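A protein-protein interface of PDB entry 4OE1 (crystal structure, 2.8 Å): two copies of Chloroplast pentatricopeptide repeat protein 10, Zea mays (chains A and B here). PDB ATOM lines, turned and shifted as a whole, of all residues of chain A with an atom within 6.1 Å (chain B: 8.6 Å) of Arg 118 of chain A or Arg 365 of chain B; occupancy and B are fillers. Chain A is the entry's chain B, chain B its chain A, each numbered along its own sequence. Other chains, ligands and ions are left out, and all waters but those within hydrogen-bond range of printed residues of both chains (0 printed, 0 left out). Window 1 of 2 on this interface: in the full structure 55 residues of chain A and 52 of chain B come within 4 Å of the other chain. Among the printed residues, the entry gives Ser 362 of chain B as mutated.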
ATOM      1  N   HIS A  86     -11.585 -11.058  -8.776  1.00  0.00           N
ATOM      2  CA  HIS A  86     -11.075 -12.243  -8.151  1.00  0.00           C
ATOM      3  C   HIS A  86     -11.954 -12.695  -7.025  1.00  0.00           C
ATOM      4  O   HIS A  86     -12.042 -13.874  -6.742  1.00  0.00           O
ATOM      5  CB  HIS A  86      -9.693 -11.950  -7.621  1.00  0.00           C
ATOM      6  CG  HIS A  86      -8.794 -11.311  -8.622  1.00  0.00           C
ATOM      7  ND1 HIS A  86      -8.253 -12.005  -9.681  1.00  0.00           N
ATOM      8  CD2 HIS A  86      -8.340 -10.045  -8.732  1.00  0.00           C
ATOM      9  CE1 HIS A  86      -7.504 -11.191 -10.397  1.00  0.00           C
ATOM     10  NE2 HIS A  86      -7.539  -9.995  -9.846  1.00  0.00           N
ATOM     11  N   LEU A 113      -7.350 -20.371  -9.707  1.00  0.00           N
ATOM     12  CA  LEU A 113      -6.107 -20.507  -8.990  1.00  0.00           C
ATOM     13  C   LEU A 113      -5.491 -19.148  -8.807  1.00  0.00           C
ATOM     14  O   LEU A 113      -4.935 -18.853  -7.766  1.00  0.00           O
ATOM     15  CB  LEU A 113      -5.153 -21.403  -9.756  1.00  0.00           C
ATOM     16  CG  LEU A 113      -5.460 -22.884  -9.855  1.00  0.00           C
ATOM     17  CD1 LEU A 113      -4.461 -23.500 -10.741  1.00  0.00           C
ATOM     18  CD2 LEU A 113      -5.380 -23.509  -8.530  1.00  0.00           C
ATOM     19  N   HIS A 114      -5.610 -18.306  -9.820  1.00  0.00           N
ATOM     20  CA  HIS A 114      -5.034 -16.980  -9.757  1.00  0.00           C
ATOM     21  C   HIS A 114      -5.830 -16.088  -8.849  1.00  0.00           C
ATOM     22  O   HIS A 114      -5.333 -15.089  -8.368  1.00  0.00           O
ATOM     23  CB  HIS A 114      -4.956 -16.343 -11.133  1.00  0.00           C
ATOM     24  CG  HIS A 114      -4.289 -15.009 -11.129  1.00  0.00           C
ATOM     25  ND1 HIS A 114      -4.951 -13.846 -11.443  1.00  0.00           N
ATOM     26  CD2 HIS A 114      -3.027 -14.645 -10.821  1.00  0.00           C
ATOM     27  CE1 HIS A 114      -4.127 -12.826 -11.338  1.00  0.00           C
ATOM     28  NE2 HIS A 114      -2.949 -13.285 -10.962  1.00  0.00           N
ATOM     29  N   ALA A 115      -7.070 -16.458  -8.614  1.00  0.00           N
ATOM     30  CA  ALA A 115      -7.941 -15.649  -7.796  1.00  0.00           C
ATOM     31  C   ALA A 115      -7.666 -15.908  -6.343  1.00  0.00           C
ATOM     32  O   ALA A 115      -7.684 -15.011  -5.531  1.00  0.00           O
ATOM     33  CB  ALA A 115      -9.356 -15.955  -8.111  1.00  0.00           C
ATOM     34  N   LEU A 116      -7.417 -17.158  -6.018  1.00  0.00           N
ATOM     35  CA  LEU A 116      -7.091 -17.533  -4.673  1.00  0.00           C
ATOM     36  C   LEU A 116      -5.729 -16.988  -4.317  1.00  0.00           C
ATOM     37  O   LEU A 116      -5.509 -16.522  -3.211  1.00  0.00           O
ATOM     38  CB  LEU A 116      -7.075 -19.043  -4.563  1.00  0.00           C
ATOM     39  CG  LEU A 116      -8.364 -19.719  -4.966  1.00  0.00           C
ATOM     40  CD1 LEU A 116      -8.094 -21.151  -5.208  1.00  0.00           C
ATOM     41  CD2 LEU A 116      -9.354 -19.566  -3.878  1.00  0.00           C
ATOM     42  N   SER A 117      -4.811 -17.066  -5.262  1.00  0.00           N
ATOM     43  CA  SER A 117      -3.475 -16.549  -5.082  1.00  0.00           C
ATOM     44  C   SER A 117      -3.576 -15.083  -4.761  1.00  0.00           C
ATOM     45  O   SER A 117      -2.969 -14.580  -3.829  1.00  0.00           O
ATOM     46  CB  SER A 117      -2.668 -16.756  -6.357  1.00  0.00           C
ATOM     47  OG  SER A 117      -1.362 -16.226  -6.266  1.00  0.00           O
ATOM     48  N   ARG A 118      -4.396 -14.405  -5.536  1.00  0.00           N
ATOM     49  CA  ARG A 118      -4.619 -12.985  -5.407  1.00  0.00           C
ATOM     50  C   ARG A 118      -5.232 -12.633  -4.055  1.00  0.00           C
ATOM     51  O   ARG A 118      -5.349 -11.474  -3.705  1.00  0.00           O
ATOM     52  CB  ARG A 118      -5.554 -12.572  -6.528  1.00  0.00           C
ATOM     53  CG  ARG A 118      -5.590 -11.118  -6.838  1.00  0.00           C
ATOM     54  CD  ARG A 118      -4.512 -10.706  -7.800  1.00  0.00           C
ATOM     55  NE  ARG A 118      -3.718  -9.641  -7.222  1.00  0.00           N
ATOM     56  CZ  ARG A 118      -4.134  -8.394  -7.082  1.00  0.00           C
ATOM     57  NH1 ARG A 118      -5.335  -8.043  -7.493  1.00  0.00           N
ATOM     58  NH2 ARG A 118      -3.345  -7.497  -6.529  1.00  0.00           N
ATOM     59  N   ALA A 119      -5.604 -13.645  -3.290  1.00  0.00           N
ATOM     60  CA  ALA A 119      -6.240 -13.436  -2.007  1.00  0.00           C
ATOM     61  C   ALA A 119      -5.419 -14.014  -0.890  1.00  0.00           C
ATOM     62  O   ALA A 119      -5.798 -13.947   0.264  1.00  0.00           O
ATOM     63  CB  ALA A 119      -7.585 -14.063  -2.002  1.00  0.00           C
ATOM     64  N   GLY A 120      -4.295 -14.612  -1.246  1.00  0.00           N
ATOM     65  CA  GLY A 120      -3.414 -15.203  -0.274  1.00  0.00           C
ATOM     66  C   GLY A 120      -3.898 -16.545   0.173  1.00  0.00           C
ATOM     67  O   GLY A 120      -3.484 -17.055   1.194  1.00  0.00           O
ATOM     68  N   ARG A 121      -4.782 -17.130  -0.598  1.00  0.00           N
ATOM     69  CA  ARG A 121      -5.280 -18.436  -0.271  1.00  0.00           C
ATOM     70  C   ARG A 121      -4.473 -19.482  -0.990  1.00  0.00           C
ATOM     71  O   ARG A 121      -4.975 -20.196  -1.833  1.00  0.00           O
ATOM     72  CB  ARG A 121      -6.753 -18.550  -0.625  1.00  0.00           C
ATOM     73  CG  ARG A 121      -7.625 -17.634   0.192  1.00  0.00           C
ATOM     74  CD  ARG A 121      -9.058 -17.722  -0.215  1.00  0.00           C
ATOM     75  NE  ARG A 121      -9.639 -19.021   0.080  1.00  0.00           N
ATOM     76  CZ  ARG A 121     -10.887 -19.345  -0.196  1.00  0.00           C
ATOM     77  NH1 ARG A 121     -11.676 -18.466  -0.775  1.00  0.00           N
ATOM     78  NH2 ARG A 121     -11.341 -20.546   0.096  1.00  0.00           N
ATOM     79  N   TYR A 122      -3.204 -19.561  -0.637  1.00  0.00           N
ATOM     80  CA  TYR A 122      -2.284 -20.443  -1.307  1.00  0.00           C
ATOM     81  C   TYR A 122      -2.621 -21.891  -1.037  1.00  0.00           C
ATOM     82  O   TYR A 122      -2.362 -22.759  -1.847  1.00  0.00           O
ATOM     83  CB  TYR A 122      -0.871 -20.159  -0.840  1.00  0.00           C
ATOM     84  CG  TYR A 122      -0.517 -18.708  -0.805  1.00  0.00           C
ATOM     85  CD1 TYR A 122      -0.430 -17.976  -1.961  1.00  0.00           C
ATOM     86  CD2 TYR A 122      -0.255 -18.072   0.384  1.00  0.00           C
ATOM     87  CE1 TYR A 122      -0.109 -16.656  -1.939  1.00  0.00           C
ATOM     88  CE2 TYR A 122       0.074 -16.754   0.418  1.00  0.00           C
ATOM     89  CZ  TYR A 122       0.144 -16.047  -0.752  1.00  0.00           C
ATOM     90  OH  TYR A 122       0.468 -14.719  -0.729  1.00  0.00           O
ATOM     91  N   ASP A 149       3.891 -19.491  -8.720  1.00  0.00           N
ATOM     92  CA  ASP A 149       3.773 -18.220  -8.029  1.00  0.00           C
ATOM     93  C   ASP A 149       3.166 -18.441  -6.658  1.00  0.00           C
ATOM     94  O   ASP A 149       3.564 -17.830  -5.689  1.00  0.00           O
ATOM     95  CB  ASP A 149       2.920 -17.261  -8.855  1.00  0.00           C
ATOM     96  CG  ASP A 149       3.241 -15.808  -8.588  1.00  0.00           C
ATOM     97  OD1 ASP A 149       4.422 -15.466  -8.443  1.00  0.00           O
ATOM     98  OD2 ASP A 149       2.308 -14.999  -8.535  1.00  0.00           O
ATOM     99  N   ARG A 153       5.011 -17.413  -2.962  1.00  0.00           N
ATOM    100  CA  ARG A 153       4.541 -16.456  -1.992  1.00  0.00           C
ATOM    101  C   ARG A 153       4.029 -17.148  -0.761  1.00  0.00           C
ATOM    102  O   ARG A 153       3.789 -16.523   0.255  1.00  0.00           O
ATOM    103  CB  ARG A 153       3.447 -15.622  -2.610  1.00  0.00           C
ATOM    104  CG  ARG A 153       3.735 -15.260  -4.032  1.00  0.00           C
ATOM    105  CD  ARG A 153       2.625 -14.445  -4.647  1.00  0.00           C
ATOM    106  NE  ARG A 153       2.983 -13.039  -4.726  1.00  0.00           N
ATOM    107  CZ  ARG A 153       3.360 -12.429  -5.834  1.00  0.00           C
ATOM    108  NH1 ARG A 153       3.427 -13.097  -6.971  1.00  0.00           N
ATOM    109  NH2 ARG A 153       3.666 -11.149  -5.801  1.00  0.00           N
ATOM    110  N   SER B 331       3.693  -4.141   5.700  1.00  0.00           N
ATOM    111  CA  SER B 331       2.744  -5.209   5.470  1.00  0.00           C
ATOM    112  C   SER B 331       3.428  -6.549   5.439  1.00  0.00           C
ATOM    113  O   SER B 331       3.144  -7.379   4.592  1.00  0.00           O
ATOM    114  CB  SER B 331       2.018  -4.995   4.157  1.00  0.00           C
ATOM    115  OG  SER B 331       2.882  -5.279   3.084  1.00  0.00           O
ATOM    116  N   PHE B 333       3.202  -9.524   6.471  1.00  0.00           N
ATOM    117  CA  PHE B 333       2.219 -10.422   7.068  1.00  0.00           C
ATOM    118  C   PHE B 333       2.798 -11.614   7.832  1.00  0.00           C
ATOM    119  O   PHE B 333       2.557 -11.766   9.029  1.00  0.00           O
ATOM    120  CB  PHE B 333       1.235 -10.915   6.007  1.00  0.00           C
ATOM    121  CG  PHE B 333       0.615  -9.812   5.203  1.00  0.00           C
ATOM    122  CD1 PHE B 333       0.364  -8.578   5.779  1.00  0.00           C
ATOM    123  CD2 PHE B 333       0.280 -10.008   3.875  1.00  0.00           C
ATOM    124  CE1 PHE B 333      -0.208  -7.560   5.043  1.00  0.00           C
ATOM    125  CE2 PHE B 333      -0.294  -8.994   3.132  1.00  0.00           C
ATOM    126  CZ  PHE B 333      -0.537  -7.766   3.717  1.00  0.00           C
ATOM    127  N   SER B 362      -1.032  -2.300   5.636  1.00  0.00           N
ATOM    128  CA  SER B 362      -1.055  -1.667   4.325  1.00  0.00           C
ATOM    129  C   SER B 362      -1.569  -2.628   3.260  1.00  0.00           C
ATOM    130  O   SER B 362      -1.058  -3.737   3.117  1.00  0.00           O
ATOM    131  CB  SER B 362       0.338  -1.169   3.956  1.00  0.00           C
ATOM    132  OG  SER B 362       1.215  -1.257   5.066  1.00  0.00           O
ATOM    133  N   GLY B 363      -2.576  -2.191   2.514  1.00  0.00           N
ATOM    134  CA  GLY B 363      -3.142  -2.999   1.450  1.00  0.00           C
ATOM    135  C   GLY B 363      -2.072  -3.653   0.603  1.00  0.00           C
ATOM    136  O   GLY B 363      -0.991  -3.093   0.409  1.00  0.00           O
ATOM    137  N   LYS B 364      -2.366  -4.846   0.098  1.00  0.00           N
ATOM    138  CA  LYS B 364      -1.409  -5.587  -0.711  1.00  0.00           C
ATOM    139  C   LYS B 364      -1.980  -6.930  -1.150  1.00  0.00           C
ATOM    140  O   LYS B 364      -3.169  -7.192  -0.991  1.00  0.00           O
ATOM    141  CB  LYS B 364      -0.106  -5.795   0.061  1.00  0.00           C
ATOM    142  CG  LYS B 364       1.059  -6.259  -0.798  1.00  0.00           C
ATOM    143  CD  LYS B 364       1.942  -7.232  -0.039  1.00  0.00           C
ATOM    144  CE  LYS B 364       3.260  -6.584   0.359  1.00  0.00           C
ATOM    145  NZ  LYS B 364       4.337  -7.598   0.552  1.00  0.00           N
ATOM    146  N   ARG B 365      -1.120  -7.772  -1.711  1.00  0.00           N
ATOM    147  CA  ARG B 365      -1.533  -9.085  -2.195  1.00  0.00           C
ATOM    148  C   ARG B 365      -1.509 -10.113  -1.072  1.00  0.00           C
ATOM    149  O   ARG B 365      -0.544 -10.199  -0.319  1.00  0.00           O
ATOM    150  CB  ARG B 365      -0.623  -9.537  -3.334  1.00  0.00           C
ATOM    151  CG  ARG B 365      -1.271 -10.515  -4.302  1.00  0.00           C
ATOM    152  CD  ARG B 365      -0.282 -11.570  -4.755  1.00  0.00           C
ATOM    153  NE  ARG B 365       0.175 -11.342  -6.121  1.00  0.00           N
ATOM    154  CZ  ARG B 365      -0.018 -12.188  -7.125  1.00  0.00           C
ATOM    155  NH1 ARG B 365      -0.662 -13.326  -6.914  1.00  0.00           N
ATOM    156  NH2 ARG B 365       0.435 -11.898  -8.335  1.00  0.00           N
ATOM    157  N   GLY B 366      -2.578 -10.900  -0.973  1.00  0.00           N
ATOM    158  CA  GLY B 366      -2.674 -11.933   0.037  1.00  0.00           C
ATOM    159  C   GLY B 366      -3.040 -11.392   1.406  1.00  0.00           C
ATOM    160  O   GLY B 366      -2.836 -12.054   2.420  1.00  0.00           O
ATOM    161  N   MET B 367      -3.589 -10.181   1.430  1.00  0.00           N
ATOM    162  CA  MET B 367      -3.969  -9.544   2.684  1.00  0.00           C
ATOM    163  C   MET B 367      -5.239 -10.155   3.264  1.00  0.00           C
ATOM    164  O   MET B 367      -5.420 -10.200   4.479  1.00  0.00           O
ATOM    165  CB  MET B 367      -4.161  -8.039   2.478  1.00  0.00           C
ATOM    166  CG  MET B 367      -4.886  -7.345   3.620  1.00  0.00           C
ATOM    167  SD  MET B 367      -4.929  -5.555   3.446  1.00  0.00           S
ATOM    168  CE  MET B 367      -5.997  -5.110   4.811  1.00  0.00           C
ATOM    169  N   GLU B 368      -6.118 -10.629   2.388  1.00  0.00           N
ATOM    170  CA  GLU B 368      -7.387 -11.204   2.812  1.00  0.00           C
ATOM    171  C   GLU B 368      -7.197 -12.412   3.724  1.00  0.00           C
ATOM    172  O   GLU B 368      -7.934 -12.584   4.693  1.00  0.00           O
ATOM    173  CB  GLU B 368      -8.228 -11.593   1.599  1.00  0.00           C
ATOM    174  CG  GLU B 368      -9.443 -12.441   1.943  1.00  0.00           C
ATOM    175  CD  GLU B 368     -10.199 -12.899   0.712  1.00  0.00           C
ATOM    176  OE1 GLU B 368     -11.149 -13.694   0.862  1.00  0.00           O
ATOM    177  OE2 GLU B 368      -9.846 -12.467  -0.402  1.00  0.00           O
ATOM    178  N   ASP B 369      -6.215 -13.246   3.408  1.00  0.00           N
ATOM    179  CA  ASP B 369      -5.968 -14.437   4.184  1.00  0.00           C
ATOM    180  C   ASP B 369      -5.326 -14.068   5.483  1.00  0.00           C
ATOM    181  O   ASP B 369      -5.520 -14.725   6.491  1.00  0.00           O
ATOM    182  CB  ASP B 369      -5.057 -15.370   3.414  1.00  0.00           C
ATOM    183  CG  ASP B 369      -4.951 -16.705   4.045  1.00  0.00           C
ATOM    184  OD1 ASP B 369      -5.971 -17.208   4.520  1.00  0.00           O
ATOM    185  OD2 ASP B 369      -3.841 -17.253   4.076  1.00  0.00           O
ATOM    186  N   TYR B 370      -4.555 -12.998   5.459  1.00  0.00           N
ATOM    187  CA  TYR B 370      -3.909 -12.501   6.647  1.00  0.00           C
ATOM    188  C   TYR B 370      -4.953 -12.090   7.647  1.00  0.00           C
ATOM    189  O   TYR B 370      -4.956 -12.554   8.767  1.00  0.00           O
ATOM    190  CB  TYR B 370      -3.019 -11.331   6.281  1.00  0.00           C
ATOM    191  CG  TYR B 370      -2.567 -10.464   7.422  1.00  0.00           C
ATOM    192  CD1 TYR B 370      -1.493 -10.806   8.206  1.00  0.00           C
ATOM    193  CD2 TYR B 370      -3.192  -9.275   7.679  1.00  0.00           C
ATOM    194  CE1 TYR B 370      -1.084  -9.998   9.218  1.00  0.00           C
ATOM    195  CE2 TYR B 370      -2.787  -8.475   8.688  1.00  0.00           C
ATOM    196  CZ  TYR B 370      -1.740  -8.832   9.450  1.00  0.00           C
ATOM    197  OH  TYR B 370      -1.365  -8.000  10.453  1.00  0.00           O
ATOM    198  N   CYS B 400      -8.872  -4.888   1.274  1.00  0.00           N
ATOM    199  CA  CYS B 400      -8.254  -5.844   0.395  1.00  0.00           C
ATOM    200  C   CYS B 400      -9.201  -6.203  -0.714  1.00  0.00           C
ATOM    201  O   CYS B 400      -8.811  -6.637  -1.761  1.00  0.00           O
ATOM    202  CB  CYS B 400      -7.827  -7.082   1.159  1.00  0.00           C
ATOM    203  SG  CYS B 400      -8.960  -7.784   2.245  1.00  0.00           S
ATOM    204  N   GLY B 401     -10.477  -6.031  -0.476  1.00  0.00           N
ATOM    205  CA  GLY B 401     -11.447  -6.221  -1.521  1.00  0.00           C
ATOM    206  C   GLY B 401     -12.245  -7.478  -1.341  1.00  0.00           C
ATOM    207  O   GLY B 401     -12.906  -7.927  -2.256  1.00  0.00           O
ATOM    208  N   SER B 402     -12.192  -8.052  -0.153  1.00  0.00           N
ATOM    209  CA  SER B 402     -12.975  -9.241   0.092  1.00  0.00           C
ATOM    210  C   SER B 402     -14.394  -8.853   0.354  1.00  0.00           C
ATOM    211  O   SER B 402     -14.847  -8.909   1.480  1.00  0.00           O
ATOM    212  CB  SER B 402     -12.452 -10.020   1.273  1.00  0.00           C
ATOM    213  OG  SER B 402     -13.233 -11.183   1.453  1.00  0.00           O
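The side-chain hydroxyl of Ser 402 of chain B lies within hydrogen-bond range of the side-chain carboxylate of Glu 368 of chain B (3.3 Å). The side-chain carboxylate (OD2) of Asp 149 of chain A lies within salt-bridge range of the guanidinium group (NH1) of Arg 153 of chain A (2.7 Å).
NH1 of Arg 365 of chain B sits at hydrogen-bond distance from OG of Ser 117 of chain A (3.1 Å). The guanidinium group of Arg 365 of chain B lies within salt-bridge range of the side-chain carboxylate of Asp 149 of chain A, 3.6 Å away. N of Asp 369 of chain B lies within hydrogen-bond range of O of Ala 119 of chain A, 3.2 Å away. The backbone carbonyl oxygen (O) of Gly 120 of chain A sits close to the side-chain carboxylate (OD2) of Asp 369 of chain B, at 2.9 Å.
Of chain B, only Arg 365 (3.1 Å) comes within 4 Å of Ser 117 of chain A. Of the printed residues of chain B, Arg 118 of chain A touches Arg 365 and Gly 366. Of the printed residues of chain B, Arg 153 of chain A touches Arg 365 (3.4 Å). Lys 364 of chain B touches none of the printed residues of chain A. Of the printed residues of chain A, Arg 365 of chain B touches Ser 117, Arg 118, Asp 149 and Arg 153. Of the printed residues of chain A, Asp 369 of chain B touches Ala 119 (3.2 Å) and Gly 120 (2.9 Å). The nearest residue of chain A that does not touch Arg 365 of chain B is His 114 of chain A (4.5 Å).
Hydrophobic or aromatic side chains of chain A within 4 Å of the printed part of chain B: Ala 119. Printed residues of chain B that touch a printed residue of chain A: Arg 365, Gly 366, Glu 368 and Asp 369. Among the printed residues, 10 pairs touch across the chains. Among the printed residues, Asp or Glu carboxylates within 4 Å of a Lys or Arg side-chain nitrogen of the other chain: Asp 149 of chain A with Arg 365 of chain B.
Among the printed residues, pairs that only touch across the chains: Ala 119 of chain A with Glu 368 of chain B (3.2 Å), Gly 120 of chain A with Gly 366 of chain B (3.4 Å), Arg 153 of chain A with Arg 365 of chain B (3.4 Å), Ala 119 of chain A with Gly 366 of chain B (3.6 Å), Arg 118 of chain A with Arg 365 of chain B (3.9 Å) and Arg 118 of chain A with Gly 366 of chain B (3.9 Å).
No position is printed for both chains. Of the 10 pairs that touch across the chains among the printed residues, none has its exchanged pair printed and touching as well.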
